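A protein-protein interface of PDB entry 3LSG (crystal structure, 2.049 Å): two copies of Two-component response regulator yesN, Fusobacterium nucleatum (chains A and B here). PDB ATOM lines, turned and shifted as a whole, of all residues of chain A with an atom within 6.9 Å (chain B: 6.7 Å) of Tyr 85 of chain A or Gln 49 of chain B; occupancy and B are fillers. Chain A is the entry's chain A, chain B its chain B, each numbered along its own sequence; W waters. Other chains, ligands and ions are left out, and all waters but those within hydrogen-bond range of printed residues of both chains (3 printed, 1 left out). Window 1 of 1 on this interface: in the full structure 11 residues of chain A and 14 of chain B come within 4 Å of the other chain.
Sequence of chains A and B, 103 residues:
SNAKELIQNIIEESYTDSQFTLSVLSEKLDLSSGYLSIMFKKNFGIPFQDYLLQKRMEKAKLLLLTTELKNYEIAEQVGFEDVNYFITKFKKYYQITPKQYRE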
ATOM      1  N   GLY A  79     -15.922 -17.682  17.189  1.00  0.00           N
ATOM      2  CA  GLY A  79     -14.513 -17.880  16.910  1.00  0.00           C
ATOM      3  C   GLY A  79     -13.783 -16.749  16.198  1.00  0.00           C
ATOM      4  O   GLY A  79     -12.711 -16.984  15.657  1.00  0.00           O
ATOM      5  N   PHE A  80     -14.339 -15.537  16.207  1.00  0.00           N
ATOM      6  CA  PHE A  80     -13.677 -14.383  15.581  1.00  0.00           C
ATOM      7  C   PHE A  80     -13.196 -13.400  16.638  1.00  0.00           C
ATOM      8  O   PHE A  80     -14.003 -12.905  17.418  1.00  0.00           O
ATOM      9  CB  PHE A  80     -14.644 -13.627  14.661  1.00  0.00           C
ATOM     10  CG  PHE A  80     -14.853 -14.276  13.335  1.00  0.00           C
ATOM     11  CD1 PHE A  80     -14.135 -13.856  12.223  1.00  0.00           C
ATOM     12  CD2 PHE A  80     -15.775 -15.304  13.186  1.00  0.00           C
ATOM     13  CE1 PHE A  80     -14.340 -14.456  10.980  1.00  0.00           C
ATOM     14  CE2 PHE A  80     -15.985 -15.896  11.963  1.00  0.00           C
ATOM     15  CZ  PHE A  80     -15.257 -15.483  10.856  1.00  0.00           C
ATOM     16  N   GLU A  81     -11.903 -13.081  16.654  1.00  0.00           N
ATOM     17  CA  GLU A  81     -11.432 -12.088  17.609  1.00  0.00           C
ATOM     18  C   GLU A  81     -11.658 -10.666  17.103  1.00  0.00           C
ATOM     19  O   GLU A  81     -11.679  -9.721  17.887  1.00  0.00           O
ATOM     20  CB  GLU A  81      -9.968 -12.329  18.051  1.00  0.00           C
ATOM     21  CG  GLU A  81      -9.065 -13.055  17.065  1.00  0.00           C
ATOM     22  CD  GLU A  81      -7.710 -13.438  17.689  1.00  0.00           C
ATOM     23  OE1 GLU A  81      -6.827 -13.981  16.969  1.00  0.00           O
ATOM     24  OE2 GLU A  81      -7.523 -13.185  18.904  1.00  0.00           O
ATOM     25  N   ASP A  82     -11.849 -10.524  15.794  1.00  0.00           N
ATOM     26  CA  ASP A  82     -12.047  -9.206  15.194  1.00  0.00           C
ATOM     27  C   ASP A  82     -13.484  -9.037  14.709  1.00  0.00           C
ATOM     28  O   ASP A  82     -13.870  -9.642  13.712  1.00  0.00           O
ATOM     29  CB  ASP A  82     -11.063  -9.019  14.028  1.00  0.00           C
ATOM     30  CG  ASP A  82     -11.056  -7.594  13.466  1.00  0.00           C
ATOM     31  OD1 ASP A  82     -12.083  -6.891  13.553  1.00  0.00           O
ATOM     32  OD2 ASP A  82     -10.005  -7.172  12.936  1.00  0.00           O
ATOM     33  N   VAL A  83     -14.268  -8.201  15.394  1.00  0.00           N
ATOM     34  CA  VAL A  83     -15.675  -8.006  15.012  1.00  0.00           C
ATOM     35  C   VAL A  83     -15.847  -7.480  13.580  1.00  0.00           C
ATOM     36  O   VAL A  83     -16.797  -7.819  12.906  1.00  0.00           O
ATOM     37  CB  VAL A  83     -16.424  -7.083  16.000  1.00  0.00           C
ATOM     38  CG1 VAL A  83     -15.770  -5.706  16.077  1.00  0.00           C
ATOM     39  CG2 VAL A  83     -17.887  -6.945  15.614  1.00  0.00           C
ATOM     40  N   ASN A  84     -14.934  -6.640  13.110  1.00  0.00           N
ATOM     41  CA  ASN A  84     -15.084  -6.124  11.755  1.00  0.00           C
ATOM     42  C   ASN A  84     -14.758  -7.161  10.694  1.00  0.00           C
ATOM     43  O   ASN A  84     -15.382  -7.187   9.637  1.00  0.00           O
ATOM     44  CB  ASN A  84     -14.269  -4.858  11.555  1.00  0.00           C
ATOM     45  CG  ASN A  84     -14.864  -3.691  12.298  1.00  0.00           C
ATOM     46  OD1 ASN A  84     -16.078  -3.481  12.264  1.00  0.00           O
ATOM     47  ND2 ASN A  84     -14.025  -2.938  12.990  1.00  0.00           N
ATOM     48  N   TYR A  85     -13.802  -8.033  10.992  1.00  0.00           N
ATOM     49  CA  TYR A  85     -13.495  -9.137  10.093  1.00  0.00           C
ATOM     50  C   TYR A  85     -14.680 -10.099  10.046  1.00  0.00           C
ATOM     51  O   TYR A  85     -15.080 -10.545   8.984  1.00  0.00           O
ATOM     52  CB  TYR A  85     -12.214  -9.864  10.514  1.00  0.00           C
ATOM     53  CG  TYR A  85     -11.664 -10.772   9.424  1.00  0.00           C
ATOM     54  CD1 TYR A  85     -11.230 -10.249   8.203  1.00  0.00           C
ATOM     55  CD2 TYR A  85     -11.585 -12.144   9.615  1.00  0.00           C
ATOM     56  CE1 TYR A  85     -10.732 -11.071   7.207  1.00  0.00           C
ATOM     57  CE2 TYR A  85     -11.082 -12.981   8.633  1.00  0.00           C
ATOM     58  CZ  TYR A  85     -10.656 -12.444   7.430  1.00  0.00           C
ATOM     59  OH  TYR A  85     -10.154 -13.288   6.457  1.00  0.00           O
ATOM     60  N   PHE A  86     -15.232 -10.419  11.209  1.00  0.00           N
ATOM     61  CA  PHE A  86     -16.497 -11.157  11.282  1.00  0.00           C
ATOM     62  C   PHE A  86     -17.587 -10.558  10.383  1.00  0.00           C
ATOM     63  O   PHE A  86     -18.232 -11.265   9.627  1.00  0.00           O
ATOM     64  CB  PHE A  86     -17.023 -11.230  12.724  1.00  0.00           C
ATOM     65  CG  PHE A  86     -18.495 -11.622  12.814  1.00  0.00           C
ATOM     66  CD1 PHE A  86     -18.913 -12.909  12.474  1.00  0.00           C
ATOM     67  CD2 PHE A  86     -19.442 -10.710  13.216  1.00  0.00           C
ATOM     68  CE1 PHE A  86     -20.260 -13.268  12.540  1.00  0.00           C
ATOM     69  CE2 PHE A  86     -20.790 -11.064  13.301  1.00  0.00           C
ATOM     70  CZ  PHE A  86     -21.196 -12.335  12.964  1.00  0.00           C
ATOM     71  N   ILE A  87     -17.782  -9.248  10.463  1.00  0.00           N
ATOM     72  CA  ILE A  87     -18.797  -8.594   9.639  1.00  0.00           C
ATOM     73  C   ILE A  87     -18.508  -8.763   8.139  1.00  0.00           C
ATOM     74  O   ILE A  87     -19.421  -9.034   7.353  1.00  0.00           O
ATOM     75  CB  ILE A  87     -18.926  -7.098  10.008  1.00  0.00           C
ATOM     76  CG1 ILE A  87     -19.712  -6.925  11.320  1.00  0.00           C
ATOM     77  CG2 ILE A  87     -19.616  -6.323   8.890  1.00  0.00           C
ATOM     78  CD1 ILE A  87     -19.475  -5.550  11.981  1.00  0.00           C
ATOM     79  N   THR A  88     -17.238  -8.635   7.743  1.00  0.00           N
ATOM     80  CA  THR A  88     -16.878  -8.810   6.341  1.00  0.00           C
ATOM     81  C   THR A  88     -17.101 -10.242   5.848  1.00  0.00           C
ATOM     82  O   THR A  88     -17.527 -10.438   4.706  1.00  0.00           O
ATOM     83  CB  THR A  88     -15.425  -8.390   6.028  1.00  0.00           C
ATOM     84  OG1 THR A  88     -14.516  -9.333   6.608  1.00  0.00           O
ATOM     85  CG2 THR A  88     -15.137  -6.994   6.559  1.00  0.00           C
ATOM     86  N   LYS A  89     -16.813 -11.239   6.685  1.00  0.00           N
ATOM     87  CA  LYS A  89     -17.042 -12.625   6.276  1.00  0.00           C
ATOM     88  C   LYS A  89     -18.546 -12.895   6.178  1.00  0.00           C
ATOM     89  O   LYS A  89     -19.008 -13.531   5.236  1.00  0.00           O
ATOM     90  CB  LYS A  89     -16.379 -13.621   7.247  1.00  0.00           C
ATOM     91  CG  LYS A  89     -14.847 -13.692   7.157  1.00  0.00           C
ATOM     92  CD  LYS A  89     -14.411 -14.239   5.803  1.00  0.00           C
ATOM     93  CE  LYS A  89     -12.945 -14.622   5.788  1.00  0.00           C
ATOM     94  NZ  LYS A  89     -12.485 -14.927   4.399  1.00  0.00           N
ATOM     95  N   PHE A  90     -19.305 -12.411   7.166  1.00  0.00           N
ATOM     96  CA  PHE A  90     -20.742 -12.612   7.199  1.00  0.00           C
ATOM     97  C   PHE A  90     -21.371 -12.009   5.946  1.00  0.00           C
ATOM     98  O   PHE A  90     -22.233 -12.620   5.305  1.00  0.00           O
ATOM     99  CB  PHE A  90     -21.343 -11.950   8.446  1.00  0.00           C
ATOM    100  CG  PHE A  90     -22.795 -12.281   8.662  1.00  0.00           C
ATOM    101  CD1 PHE A  90     -23.170 -13.282   9.551  1.00  0.00           C
ATOM    102  CD2 PHE A  90     -23.783 -11.597   7.974  1.00  0.00           C
ATOM    103  CE1 PHE A  90     -24.522 -13.598   9.749  1.00  0.00           C
ATOM    104  CE2 PHE A  90     -25.128 -11.896   8.178  1.00  0.00           C
ATOM    105  CZ  PHE A  90     -25.498 -12.901   9.055  1.00  0.00           C
ATOM    106  N   LYS A  91     -20.945 -10.799   5.602  1.00  0.00           N
ATOM    107  CA  LYS A  91     -21.508 -10.120   4.452  1.00  0.00           C
ATOM    108  C   LYS A  91     -21.161 -10.854   3.154  1.00  0.00           C
ATOM    109  O   LYS A  91     -21.942 -10.881   2.220  1.00  0.00           O
ATOM    110  CB  LYS A  91     -21.048  -8.663   4.371  1.00  0.00           C
ATOM    111  CG  LYS A  91     -21.711  -7.932   3.196  1.00  0.00           C
ATOM    112  CD  LYS A  91     -21.495  -6.435   3.229  1.00  0.00           C
ATOM    113  CE  LYS A  91     -22.179  -5.784   2.036  1.00  0.00           C
ATOM    114  NZ  LYS A  91     -21.810  -4.356   1.885  1.00  0.00           N
ATOM    115  N   LYS A  92     -19.983 -11.444   3.084  1.00  0.00           N
ATOM    116  CA  LYS A  92     -19.637 -12.208   1.883  1.00  0.00           C
ATOM    117  C   LYS A  92     -20.451 -13.493   1.828  1.00  0.00           C
ATOM    118  O   LYS A  92     -20.849 -13.944   0.748  1.00  0.00           O
ATOM    119  CB  LYS A  92     -18.144 -12.530   1.843  1.00  0.00           C
ATOM    120  CG  LYS A  92     -17.274 -11.340   1.460  1.00  0.00           C
ATOM    121  CD  LYS A  92     -15.923 -11.819   0.947  1.00  0.00           C
ATOM    122  CE  LYS A  92     -14.894 -10.703   0.936  1.00  0.00           C
ATOM    123  NZ  LYS A  92     -14.431 -10.373   2.311  1.00  0.00           N
ATOM    124  N   THR B  21      -1.194 -14.518  14.270  1.00  0.00           N
ATOM    125  CA  THR B  21      -2.596 -14.116  14.308  1.00  0.00           C
ATOM    126  C   THR B  21      -2.773 -12.816  15.080  1.00  0.00           C
ATOM    127  O   THR B  21      -1.843 -12.302  15.694  1.00  0.00           O
ATOM    128  CB  THR B  21      -3.440 -15.136  15.053  1.00  0.00           C
ATOM    129  OG1 THR B  21      -2.993 -15.193  16.414  1.00  0.00           O
ATOM    130  CG2 THR B  21      -3.316 -16.513  14.421  1.00  0.00           C
ATOM    131  N   LEU B  22      -3.995 -12.312  15.083  1.00  0.00           N
ATOM    132  CA  LEU B  22      -4.277 -11.057  15.748  1.00  0.00           C
ATOM    133  C   LEU B  22      -3.888 -11.158  17.228  1.00  0.00           C
ATOM    134  O   LEU B  22      -3.372 -10.202  17.801  1.00  0.00           O
ATOM    135  CB  LEU B  22      -5.755 -10.688  15.571  1.00  0.00           C
ATOM    136  CG  LEU B  22      -6.253  -9.455  16.309  1.00  0.00           C
ATOM    137  CD1 LEU B  22      -5.537  -8.225  15.807  1.00  0.00           C
ATOM    138  CD2 LEU B  22      -7.742  -9.331  16.119  1.00  0.00           C
ATOM    139  N   PHE B  40      -6.595  -0.955  15.064  1.00  0.00           N
ATOM    140  CA  PHE B  40      -5.966  -1.315  13.786  1.00  0.00           C
ATOM    141  C   PHE B  40      -6.759  -0.807  12.568  1.00  0.00           C
ATOM    142  O   PHE B  40      -6.209  -0.176  11.660  1.00  0.00           O
ATOM    143  CB  PHE B  40      -5.742  -2.826  13.674  1.00  0.00           C
ATOM    144  CG  PHE B  40      -4.900  -3.209  12.484  1.00  0.00           C
ATOM    145  CD1 PHE B  40      -3.523  -3.320  12.602  1.00  0.00           C
ATOM    146  CD2 PHE B  40      -5.482  -3.418  11.235  1.00  0.00           C
ATOM    147  CE1 PHE B  40      -2.725  -3.646  11.495  1.00  0.00           C
ATOM    148  CE2 PHE B  40      -4.696  -3.748  10.126  1.00  0.00           C
ATOM    149  CZ  PHE B  40      -3.312  -3.859  10.260  1.00  0.00           C
ATOM    150  N   ILE B  46      -8.496  -1.104   7.026  1.00  0.00           N
ATOM    151  CA  ILE B  46      -9.031  -2.449   6.867  1.00  0.00           C
ATOM    152  C   ILE B  46      -8.688  -3.273   8.101  1.00  0.00           C
ATOM    153  O   ILE B  46      -7.790  -2.914   8.853  1.00  0.00           O
ATOM    154  CB  ILE B  46      -8.437  -3.146   5.633  1.00  0.00           C
ATOM    155  CG1 ILE B  46      -6.918  -3.257   5.767  1.00  0.00           C
ATOM    156  CG2 ILE B  46      -8.819  -2.377   4.349  1.00  0.00           C
ATOM    157  CD1 ILE B  46      -6.207  -3.737   4.489  1.00  0.00           C
ATOM    158  N   PRO B  47      -9.408  -4.377   8.322  1.00  0.00           N
ATOM    159  CA  PRO B  47      -9.081  -5.261   9.446  1.00  0.00           C
ATOM    160  C   PRO B  47      -7.683  -5.871   9.321  1.00  0.00           C
ATOM    161  O   PRO B  47      -7.177  -6.071   8.211  1.00  0.00           O
ATOM    162  CB  PRO B  47     -10.142  -6.362   9.349  1.00  0.00           C
ATOM    163  CG  PRO B  47     -11.262  -5.748   8.574  1.00  0.00           C
ATOM    164  CD  PRO B  47     -10.607  -4.825   7.591  1.00  0.00           C
ATOM    165  N   PHE B  48      -7.081  -6.177  10.465  1.00  0.00           N
ATOM    166  CA  PHE B  48      -5.760  -6.811  10.519  1.00  0.00           C
ATOM    167  C   PHE B  48      -5.630  -8.031   9.597  1.00  0.00           C
ATOM    168  O   PHE B  48      -4.657  -8.160   8.861  1.00  0.00           O
ATOM    169  CB  PHE B  48      -5.412  -7.197  11.962  1.00  0.00           C
ATOM    170  CG  PHE B  48      -4.324  -8.230  12.068  1.00  0.00           C
ATOM    171  CD1 PHE B  48      -2.990  -7.869  11.956  1.00  0.00           C
ATOM    172  CD2 PHE B  48      -4.632  -9.563  12.258  1.00  0.00           C
ATOM    173  CE1 PHE B  48      -1.987  -8.828  12.037  1.00  0.00           C
ATOM    174  CE2 PHE B  48      -3.627 -10.528  12.342  1.00  0.00           C
ATOM    175  CZ  PHE B  48      -2.315 -10.157  12.237  1.00  0.00           C
ATOM    176  N   GLN B  49      -6.613  -8.921   9.629  1.00  0.00           N
ATOM    177  CA  GLN B  49      -6.534 -10.149   8.837  1.00  0.00           C
ATOM    178  C   GLN B  49      -6.483  -9.883   7.339  1.00  0.00           C
ATOM    179  O   GLN B  49      -5.794 -10.588   6.581  1.00  0.00           O
ATOM    180  CB  GLN B  49      -7.669 -11.103   9.220  1.00  0.00           C
ATOM    181  CG  GLN B  49      -7.337 -11.849  10.484  1.00  0.00           C
ATOM    182  CD  GLN B  49      -8.544 -12.405  11.202  1.00  0.00           C
ATOM    183  OE1 GLN B  49      -8.820 -13.601  11.131  1.00  0.00           O
ATOM    184  NE2 GLN B  49      -9.263 -11.542  11.907  1.00  0.00           N
ATOM    185  N   ASP B  50      -7.180  -8.839   6.912  1.00  0.00           N
ATOM    186  CA  ASP B  50      -7.086  -8.418   5.517  1.00  0.00           C
ATOM    187  C   ASP B  50      -5.737  -7.805   5.204  1.00  0.00           C
ATOM    188  O   ASP B  50      -5.188  -8.048   4.138  1.00  0.00           O
ATOM    189  CB  ASP B  50      -8.223  -7.474   5.151  1.00  0.00           C
ATOM    190  CG  ASP B  50      -9.541  -8.208   5.002  1.00  0.00           C
ATOM    191  OD1 ASP B  50      -9.530  -9.306   4.409  1.00  0.00           O
ATOM    192  OD2 ASP B  50     -10.570  -7.705   5.488  1.00  0.00           O
ATOM    193  N   TYR B  51      -5.188  -7.026   6.135  1.00  0.00           N
ATOM    194  CA  TYR B  51      -3.857  -6.460   5.921  1.00  0.00           C
ATOM    195  C   TYR B  51      -2.822  -7.577   5.864  1.00  0.00           C
ATOM    196  O   TYR B  51      -1.909  -7.555   5.044  1.00  0.00           O
ATOM    197  CB  TYR B  51      -3.497  -5.494   7.044  1.00  0.00           C
ATOM    198  CG  TYR B  51      -2.162  -4.793   6.856  1.00  0.00           C
ATOM    199  CD1 TYR B  51      -2.072  -3.605   6.132  1.00  0.00           C
ATOM    200  CD2 TYR B  51      -0.990  -5.312   7.415  1.00  0.00           C
ATOM    201  CE1 TYR B  51      -0.847  -2.951   5.956  1.00  0.00           C
ATOM    202  CE2 TYR B  51       0.254  -4.659   7.249  1.00  0.00           C
ATOM    203  CZ  TYR B  51       0.307  -3.485   6.523  1.00  0.00           C
ATOM    204  OH  TYR B  51       1.515  -2.853   6.353  1.00  0.00           O
ATOM    205  N   LEU B  52      -2.945  -8.536   6.767  1.00  0.00           N
ATOM    206  CA  LEU B  52      -2.048  -9.682   6.778  1.00  0.00           C
ATOM    207  C   LEU B  52      -2.115 -10.428   5.443  1.00  0.00           C
ATOM    208  O   LEU B  52      -1.090 -10.759   4.861  1.00  0.00           O
ATOM    209  CB  LEU B  52      -2.380 -10.619   7.941  1.00  0.00           C
ATOM    210  CG  LEU B  52      -1.574 -11.925   8.023  1.00  0.00           C
ATOM    211  CD1 LEU B  52      -0.068 -11.657   8.145  1.00  0.00           C
ATOM    212  CD2 LEU B  52      -2.067 -12.801   9.171  1.00  0.00           C
ATOM    213  N   LEU B  53      -3.319 -10.702   4.960  1.00  0.00           N
ATOM    214  CA  LEU B  53      -3.465 -11.351   3.662  1.00  0.00           C
ATOM    215  C   LEU B  53      -2.737 -10.543   2.594  1.00  0.00           C
ATOM    216  O   LEU B  53      -2.003 -11.091   1.766  1.00  0.00           O
ATOM    217  CB  LEU B  53      -4.934 -11.504   3.282  1.00  0.00           C
ATOM    218  CG  LEU B  53      -5.198 -11.970   1.845  1.00  0.00           C
ATOM    219  CD1 LEU B  53      -4.603 -13.355   1.618  1.00  0.00           C
ATOM    220  CD2 LEU B  53      -6.707 -11.981   1.567  1.00  0.00           C
ATOM    221  N   GLN B  54      -2.930  -9.233   2.616  1.00  0.00           N
ATOM    222  CA  GLN B  54      -2.293  -8.377   1.623  1.00  0.00           C
ATOM    223  C   GLN B  54      -0.768  -8.540   1.584  1.00  0.00           C
ATOM    224  O   GLN B  54      -0.186  -8.682   0.512  1.00  0.00           O
ATOM    225  CB  GLN B  54      -2.668  -6.918   1.857  1.00  0.00           C
ATOM    226  CG  GLN B  54      -1.942  -5.942   0.942  1.00  0.00           C
ATOM    227  CD  GLN B  54      -2.188  -4.496   1.352  1.00  0.00           C
ATOM    228  OE1 GLN B  54      -3.287  -4.140   1.789  1.00  0.00           O
ATOM    229  NE2 GLN B  54      -1.161  -3.661   1.222  1.00  0.00           N
ATOM    230  N   TYR B  85      -5.404 -23.882  -0.384  1.00  0.00           N
ATOM    231  CA  TYR B  85      -5.980 -22.645   0.127  1.00  0.00           C
ATOM    232  C   TYR B  85      -5.212 -21.431  -0.392  1.00  0.00           C
ATOM    233  O   TYR B  85      -5.810 -20.411  -0.732  1.00  0.00           O
ATOM    234  CB  TYR B  85      -6.026 -22.617   1.652  1.00  0.00           C
ATOM    235  CG  TYR B  85      -7.060 -21.625   2.169  1.00  0.00           C
ATOM    236  CD1 TYR B  85      -8.345 -21.620   1.645  1.00  0.00           C
ATOM    237  CD2 TYR B  85      -6.753 -20.708   3.170  1.00  0.00           C
ATOM    238  CE1 TYR B  85      -9.308 -20.717   2.097  1.00  0.00           C
ATOM    239  CE2 TYR B  85      -7.710 -19.809   3.636  1.00  0.00           C
ATOM    240  CZ  TYR B  85      -8.984 -19.823   3.084  1.00  0.00           C
ATOM    241  OH  TYR B  85      -9.950 -18.949   3.523  1.00  0.00           O
ATOM    242  N   LYS B  89      -6.802 -18.490  -2.547  1.00  0.00           N
ATOM    243  CA  LYS B  89      -6.781 -17.127  -2.040  1.00  0.00           C
ATOM    244  C   LYS B  89      -6.090 -16.199  -3.032  1.00  0.00           C
ATOM    245  O   LYS B  89      -6.503 -15.053  -3.212  1.00  0.00           O
ATOM    246  CB  LYS B  89      -6.130 -17.047  -0.658  1.00  0.00           C
ATOM    247  CG  LYS B  89      -6.993 -17.644   0.435  1.00  0.00           C
ATOM    248  CD  LYS B  89      -8.263 -16.823   0.630  1.00  0.00           C
ATOM    249  CE  LYS B  89      -7.977 -15.619   1.511  1.00  0.00           C
ATOM    250  NZ  LYS B  89      -9.236 -15.013   2.029  1.00  0.00           N
HETATM  251  O   HOH W   1      -8.334  -9.092  11.777  1.00  0.00           O
HETATM  252  O   HOH W   2      -8.416  -5.286  12.895  1.00  0.00           O
HETATM  253  O   HOH W   3      -8.852 -12.409   4.343  1.00  0.00           O
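The backbone carbonyl oxygen (O) of Tyr 85 of chain A sits at hydrogen-bond distance from the side-chain hydroxyl (OG1) of Thr 88 of chain A. The side-chain carboxylate of Asp 82 of chain A lies within hydrogen-bond range of the backbone NH of Tyr 85 of chain A (3.3 Å). The side-chain carboxylate (OD1) of Asp 82 of chain A sits at hydrogen-bond distance from the backbone NH (N) of Asn 84 of chain A, at 2.9 Å.
Among the printed residues, pairs that only touch across the chains: Glu 81 of chain A with Leu 22 of chain B (3.7 Å), Asp 82 of chain A with Leu 22 of chain B (3.9 Å), Asp 82 of chain A with Pro 47 of chain B (3.7 Å), Asp 82 of chain A with Phe 48 of chain B (3.96 Å), Asp 82 of chain A with Gln 49 of chain B (3.8 Å), Tyr 85 of chain A with Gln 49 of chain B (3.3 Å) and Tyr 85 of chain A with Asp 50 of chain B (3.5 Å).
Tyr 85 of chain A touches just these residues of chain B: Gln 49 and Asp 50. Gln 49 of chain B touches just these residues of chain A: Asp 82 and Tyr 85. Of the printed residues of chain A, Phe 48 of chain B touches Asp 82 (3.96 Å). Printed residues of chain A within 4 Å of Asp 50 of chain B: Tyr 85. Of the printed residues of chain A, Leu 22 of chain B touches Glu 81 (3.7 Å) and Asp 82 (3.9 Å). Printed residues of chain A within 4 Å of Pro 47 of chain B: Asp 82 (3.7 Å). Ile 46 of chain B touches none of the printed residues of chain A. The nearest residue of chain B that does not touch Tyr 85 of chain A is Pro 47 of chain B (4.2 Å). The nearest printed residue of chain A that does not touch Phe 48 of chain B is Tyr 85 of chain A (6.2 Å).
Of the 14 printed residues of chain A, 3 touch a printed residue of chain B. Hydrophobic or aromatic side chains of chain A within 4 Å of the printed part of chain B: Tyr 85. Of the 14 printed residues of chain B, 5 touch a printed residue of chain A. Printed residues of chain B that touch a printed residue of chain A: Leu 22, Pro 47, Phe 48, Gln 49 and Asp 50. Hydrophobic or aromatic side chains of chain B within 4 Å of the printed part of chain A: Leu 22 and Pro 47. Among the printed residues, 7 pairs touch across the chains. Among the printed residues, no Asp or Glu carboxylate lies within 4 Å of a Lys or Arg side-chain nitrogen of the other chain.
2 positions are printed for both chains.
Water W2 lies within hydrogen-bond range of OD2 of Asp 82 of chain A and N of Phe 48 of chain B. Water W1 lies within hydrogen-bond range of the side-chain amide nitrogen of Gln 49 of chain B (2.6 Å), the side-chain carboxylate of Asp 82 of chain A (2.8 Å) and the backbone NH of Phe 48 of chain B (3.4 Å). Water W3 bridges the side-chain hydroxyl (OH) of Tyr 85 of chain A (2.6 Å) and the side-chain carboxylate (OD1) of Asp 50 of chain B (3.2 Å).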
